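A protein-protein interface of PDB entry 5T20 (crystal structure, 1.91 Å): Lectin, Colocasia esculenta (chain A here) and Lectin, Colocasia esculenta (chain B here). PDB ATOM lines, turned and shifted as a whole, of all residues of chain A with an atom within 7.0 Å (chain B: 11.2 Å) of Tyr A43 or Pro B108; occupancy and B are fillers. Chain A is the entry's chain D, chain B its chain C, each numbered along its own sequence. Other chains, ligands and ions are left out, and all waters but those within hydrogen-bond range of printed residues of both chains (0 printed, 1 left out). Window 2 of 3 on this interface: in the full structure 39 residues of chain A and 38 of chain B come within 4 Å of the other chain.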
ATOM      1  N   LEU A  38     -12.317 -24.284  24.039  1.00  0.00           N
ATOM      2  CA  LEU A  38     -11.146 -23.751  23.374  1.00  0.00           C
ATOM      3  C   LEU A  38     -11.389 -22.265  23.153  1.00  0.00           C
ATOM      4  O   LEU A  38     -12.244 -21.911  22.345  1.00  0.00           O
ATOM      5  CB  LEU A  38     -10.818 -24.467  22.048  1.00  0.00           C
ATOM      6  CG  LEU A  38      -9.341 -24.363  21.602  1.00  0.00           C
ATOM      7  CD1 LEU A  38      -9.026 -25.385  20.496  1.00  0.00           C
ATOM      8  CD2 LEU A  38      -8.996 -22.970  21.122  1.00  0.00           C
ATOM      9  N   GLY A  40      -9.944 -19.177  21.604  1.00  0.00           N
ATOM     10  CA  GLY A  40      -8.951 -18.823  20.599  1.00  0.00           C
ATOM     11  C   GLY A  40      -9.485 -19.063  19.204  1.00  0.00           C
ATOM     12  O   GLY A  40     -10.688 -19.284  19.033  1.00  0.00           O
ATOM     13  N   GLY A  41      -8.595 -18.991  18.212  1.00  0.00           N
ATOM     14  CA  GLY A  41      -9.001 -19.131  16.818  1.00  0.00           C
ATOM     15  C   GLY A  41      -9.809 -17.905  16.447  1.00  0.00           C
ATOM     16  O   GLY A  41      -9.426 -16.793  16.827  1.00  0.00           O
ATOM     17  N   LYS A  42     -10.948 -18.098  15.743  1.00  0.00           N
ATOM     18  CA  LYS A  42     -11.872 -17.020  15.355  1.00  0.00           C
ATOM     19  C   LYS A  42     -13.207 -17.154  16.105  1.00  0.00           C
ATOM     20  O   LYS A  42     -13.763 -16.152  16.560  1.00  0.00           O
ATOM     21  CB  LYS A  42     -12.108 -17.045  13.822  1.00  0.00           C
ATOM     22  CG  LYS A  42     -13.204 -16.107  13.286  1.00  0.00           C
ATOM     23  CD  LYS A  42     -12.681 -14.727  12.927  1.00  0.00           C
ATOM     24  CE  LYS A  42     -13.770 -13.825  12.391  1.00  0.00           C
ATOM     25  NZ  LYS A  42     -13.284 -12.432  12.204  1.00  0.00           N
ATOM     26  N   TYR A  43     -13.743 -18.379  16.180  1.00  0.00           N
ATOM     27  CA  TYR A  43     -15.031 -18.665  16.810  1.00  0.00           C
ATOM     28  C   TYR A  43     -14.892 -19.390  18.138  1.00  0.00           C
ATOM     29  O   TYR A  43     -15.867 -19.522  18.894  1.00  0.00           O
ATOM     30  CB  TYR A  43     -15.850 -19.575  15.862  1.00  0.00           C
ATOM     31  CG  TYR A  43     -16.169 -18.955  14.521  1.00  0.00           C
ATOM     32  CD1 TYR A  43     -17.303 -18.166  14.349  1.00  0.00           C
ATOM     33  CD2 TYR A  43     -15.376 -19.213  13.405  1.00  0.00           C
ATOM     34  CE1 TYR A  43     -17.626 -17.623  13.105  1.00  0.00           C
ATOM     35  CE2 TYR A  43     -15.681 -18.665  12.158  1.00  0.00           C
ATOM     36  CZ  TYR A  43     -16.814 -17.878  12.011  1.00  0.00           C
ATOM     37  OH  TYR A  43     -17.134 -17.342  10.788  1.00  0.00           O
ATOM     38  N   GLY A  44     -13.701 -19.918  18.386  1.00  0.00           N
ATOM     39  CA  GLY A  44     -13.478 -20.761  19.545  1.00  0.00           C
ATOM     40  C   GLY A  44     -14.150 -22.103  19.312  1.00  0.00           C
ATOM     41  O   GLY A  44     -14.592 -22.411  18.193  1.00  0.00           O
ATOM     42  N   TRP A  45     -14.236 -22.912  20.372  1.00  0.00           N
ATOM     43  CA  TRP A  45     -14.898 -24.212  20.328  1.00  0.00           C
ATOM     44  C   TRP A  45     -15.319 -24.600  21.723  1.00  0.00           C
ATOM     45  O   TRP A  45     -14.699 -24.179  22.707  1.00  0.00           O
ATOM     46  CB  TRP A  45     -13.965 -25.285  19.716  1.00  0.00           C
ATOM     47  CG  TRP A  45     -14.555 -26.677  19.622  1.00  0.00           C
ATOM     48  CD1 TRP A  45     -15.196 -27.228  18.549  1.00  0.00           C
ATOM     49  CD2 TRP A  45     -14.499 -27.707  20.631  1.00  0.00           C
ATOM     50  NE1 TRP A  45     -15.485 -28.554  18.800  1.00  0.00           N
ATOM     51  CE2 TRP A  45     -15.088 -28.868  20.076  1.00  0.00           C
ATOM     52  CE3 TRP A  45     -13.927 -27.787  21.921  1.00  0.00           C
ATOM     53  CZ2 TRP A  45     -15.203 -30.066  20.792  1.00  0.00           C
ATOM     54  CZ3 TRP A  45     -14.027 -28.980  22.629  1.00  0.00           C
ATOM     55  CH2 TRP A  45     -14.674 -30.097  22.075  1.00  0.00           C
ATOM     56  N   GLN A  46     -16.395 -25.380  21.816  1.00  0.00           N
ATOM     57  CA  GLN A  46     -16.843 -25.912  23.097  1.00  0.00           C
ATOM     58  C   GLN A  46     -17.415 -27.309  22.904  1.00  0.00           C
ATOM     59  O   GLN A  46     -17.936 -27.640  21.821  1.00  0.00           O
ATOM     60  CB  GLN A  46     -17.843 -24.983  23.812  1.00  0.00           C
ATOM     61  CG  GLN A  46     -19.158 -24.723  23.056  1.00  0.00           C
ATOM     62  CD  GLN A  46     -20.263 -24.149  23.917  1.00  0.00           C
ATOM     63  OE1 GLN A  46     -20.310 -24.338  25.127  1.00  0.00           O
ATOM     64  NE2 GLN A  46     -21.255 -23.529  23.291  1.00  0.00           N
ATOM     65  N   LYS B 102      -9.147 -33.575  15.369  1.00  0.00           N
ATOM     66  CA  LYS B 102      -8.788 -32.155  15.368  1.00  0.00           C
ATOM     67  C   LYS B 102      -9.949 -31.292  15.850  1.00  0.00           C
ATOM     68  O   LYS B 102     -11.086 -31.476  15.411  1.00  0.00           O
ATOM     69  CB  LYS B 102      -8.407 -31.751  13.923  1.00  0.00           C
ATOM     70  CG  LYS B 102      -7.928 -30.308  13.738  1.00  0.00           C
ATOM     71  CD  LYS B 102      -7.071 -30.154  12.471  1.00  0.00           C
ATOM     72  CE  LYS B 102      -7.859 -29.761  11.246  1.00  0.00           C
ATOM     73  NZ  LYS B 102      -6.976 -29.563  10.065  1.00  0.00           N
ATOM     74  N   ILE B 103      -9.658 -30.356  16.754  1.00  0.00           N
ATOM     75  CA  ILE B 103     -10.601 -29.344  17.191  1.00  0.00           C
ATOM     76  C   ILE B 103     -10.280 -28.123  16.329  1.00  0.00           C
ATOM     77  O   ILE B 103      -9.120 -27.690  16.297  1.00  0.00           O
ATOM     78  CB  ILE B 103     -10.543 -29.057  18.712  1.00  0.00           C
ATOM     79  CG1 ILE B 103     -11.085 -30.257  19.530  1.00  0.00           C
ATOM     80  CG2 ILE B 103     -11.355 -27.795  19.028  1.00  0.00           C
ATOM     81  CD1 ILE B 103     -10.682 -30.275  21.020  1.00  0.00           C
ATOM     82  N   ASP B 104     -11.286 -27.596  15.614  1.00  0.00           N
ATOM     83  CA  ASP B 104     -11.107 -26.470  14.716  1.00  0.00           C
ATOM     84  C   ASP B 104     -11.835 -25.226  15.266  1.00  0.00           C
ATOM     85  O   ASP B 104     -13.042 -25.116  15.093  1.00  0.00           O
ATOM     86  CB  ASP B 104     -11.588 -26.837  13.286  1.00  0.00           C
ATOM     87  CG  ASP B 104     -11.366 -25.788  12.189  1.00  0.00           C
ATOM     88  OD1 ASP B 104     -10.903 -24.662  12.510  1.00  0.00           O
ATOM     89  OD2 ASP B 104     -11.634 -26.098  11.012  1.00  0.00           O
ATOM     90  N   PRO B 105     -11.115 -24.267  15.909  1.00  0.00           N
ATOM     91  CA  PRO B 105     -11.785 -23.036  16.400  1.00  0.00           C
ATOM     92  C   PRO B 105     -11.820 -21.911  15.344  1.00  0.00           C
ATOM     93  O   PRO B 105     -12.151 -20.763  15.663  1.00  0.00           O
ATOM     94  CB  PRO B 105     -10.909 -22.628  17.582  1.00  0.00           C
ATOM     95  CG  PRO B 105      -9.511 -23.052  17.148  1.00  0.00           C
ATOM     96  CD  PRO B 105      -9.668 -24.256  16.227  1.00  0.00           C
ATOM     97  N   TRP B 106     -11.430 -22.224  14.096  1.00  0.00           N
ATOM     98  CA  TRP B 106     -11.389 -21.253  12.987  1.00  0.00           C
ATOM     99  C   TRP B 106     -12.654 -21.310  12.143  1.00  0.00           C
ATOM    100  O   TRP B 106     -12.942 -20.373  11.399  1.00  0.00           O
ATOM    101  CB  TRP B 106     -10.188 -21.504  12.089  1.00  0.00           C
ATOM    102  CG  TRP B 106      -8.889 -21.365  12.807  1.00  0.00           C
ATOM    103  CD1 TRP B 106      -8.123 -22.369  13.320  1.00  0.00           C
ATOM    104  CD2 TRP B 106      -8.280 -20.147  13.211  1.00  0.00           C
ATOM    105  NE1 TRP B 106      -7.018 -21.845  13.942  1.00  0.00           N
ATOM    106  CE2 TRP B 106      -7.112 -20.480  13.931  1.00  0.00           C
ATOM    107  CE3 TRP B 106      -8.620 -18.793  13.056  1.00  0.00           C
ATOM    108  CZ2 TRP B 106      -6.252 -19.510  14.444  1.00  0.00           C
ATOM    109  CZ3 TRP B 106      -7.754 -17.832  13.553  1.00  0.00           C
ATOM    110  CH2 TRP B 106      -6.602 -18.195  14.257  1.00  0.00           C
ATOM    111  N   VAL B 107     -13.378 -22.431  12.247  1.00  0.00           N
ATOM    112  CA  VAL B 107     -14.621 -22.756  11.536  1.00  0.00           C
ATOM    113  C   VAL B 107     -15.649 -23.198  12.615  1.00  0.00           C
ATOM    114  O   VAL B 107     -15.288 -24.015  13.472  1.00  0.00           O
ATOM    115  CB  VAL B 107     -14.320 -23.862  10.479  1.00  0.00           C
ATOM    116  CG1 VAL B 107     -15.586 -24.471   9.900  1.00  0.00           C
ATOM    117  CG2 VAL B 107     -13.413 -23.339   9.365  1.00  0.00           C
ATOM    118  N   PRO B 108     -16.915 -22.690  12.573  1.00  0.00           N
ATOM    119  CA  PRO B 108     -17.901 -23.011  13.626  1.00  0.00           C
ATOM    120  C   PRO B 108     -18.021 -24.482  14.052  1.00  0.00           C
ATOM    121  O   PRO B 108     -18.341 -24.734  15.221  1.00  0.00           O
ATOM    122  CB  PRO B 108     -19.216 -22.527  13.019  1.00  0.00           C
ATOM    123  CG  PRO B 108     -18.831 -21.372  12.202  1.00  0.00           C
ATOM    124  CD  PRO B 108     -17.469 -21.696  11.628  1.00  0.00           C
ATOM    125  N   GLY B 109     -17.743 -25.420  13.140  1.00  0.00           N
ATOM    126  CA  GLY B 109     -17.790 -26.854  13.420  1.00  0.00           C
ATOM    127  C   GLY B 109     -16.861 -27.344  14.521  1.00  0.00           C
ATOM    128  O   GLY B 109     -15.812 -26.750  14.796  1.00  0.00           O
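The backbone NH (N) of Trp B106 lies within hydrogen-bond range of the side-chain carboxylate (OD1) of Asp B104 (3.0 Å).
The side-chain carboxylate (OD1) of Asp B104 sits at hydrogen-bond distance from the backbone NH (N) of Val B107 (3.3 Å).
O of Trp A45 is in hydrogen-bond range of N of Leu A38, at 2.7 Å.
Hydrophobic or aromatic side chains of chain A that line the printed part of chain B: Leu A38, Tyr A43 and Trp A45.
Printed residues of chain B that touch a printed residue of chain A: Ile B103, Pro B105, Trp B106, Val B107, Pro B108 and Gly B109.
Along chain B the printed residues that touch a printed residue of chain A span positions 103 to 109.
Among the printed residues, pairs that only touch across the chains: Leu A38 with Ile B103, Gly A40 with Pro B105, Gly A41 with Pro B105, Gly A41 with Trp B106, Lys A42 with Trp B106, Tyr A43 with Trp B106, Tyr A43 with Val B107, Tyr A43 with Pro B108, Trp A45 with Ile B103 and Trp A45 with Gly B109.
Gly A40 touches just one residue of chain B: Pro B105 (3.7 Å).
Of chain B, only Pro B105 and Trp B106 come within 4 Å of Gly A41.
Of the printed residues of chain B, Lys A42 touches Pro B105 and Trp B106.
Of chain B, only Pro B105 (3.2 Å) comes within 4 Å of Gly A44.
Gln A46 touches none of the printed residues of chain B.
Lys B102 touches none of the printed residues of chain A.
Of the printed residues of chain A, Ile B103 touches Leu A38 (3.7 Å) and Trp A45 (3.4 Å).
Printed residues of chain A within 4 Å of Pro B105: Gly A40 (3.7 Å), Gly A41 (3.7 Å), Lys A42 (2.9 Å), Tyr A43 (2.9 Å) and Gly A44 (3.2 Å).
Pro B108 touches just one residue of chain A: Tyr A43.
The nearest residue of chain B that does not touch Tyr A43 is Asp B104 (6.3 Å).
The nearest residue of chain A that does not touch Pro B108 is Trp A45 (5.2 Å).
O of Pro B105 is in hydrogen-bond range of N of Lys A42, 2.9 Å away.
O of Pro B105 is in hydrogen-bond range of N of Tyr A43 (2.9 Å).
The backbone NH of Gly A44 is in hydrogen-bond range of the backbone carbonyl oxygen of Pro B105 (3.2 Å).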
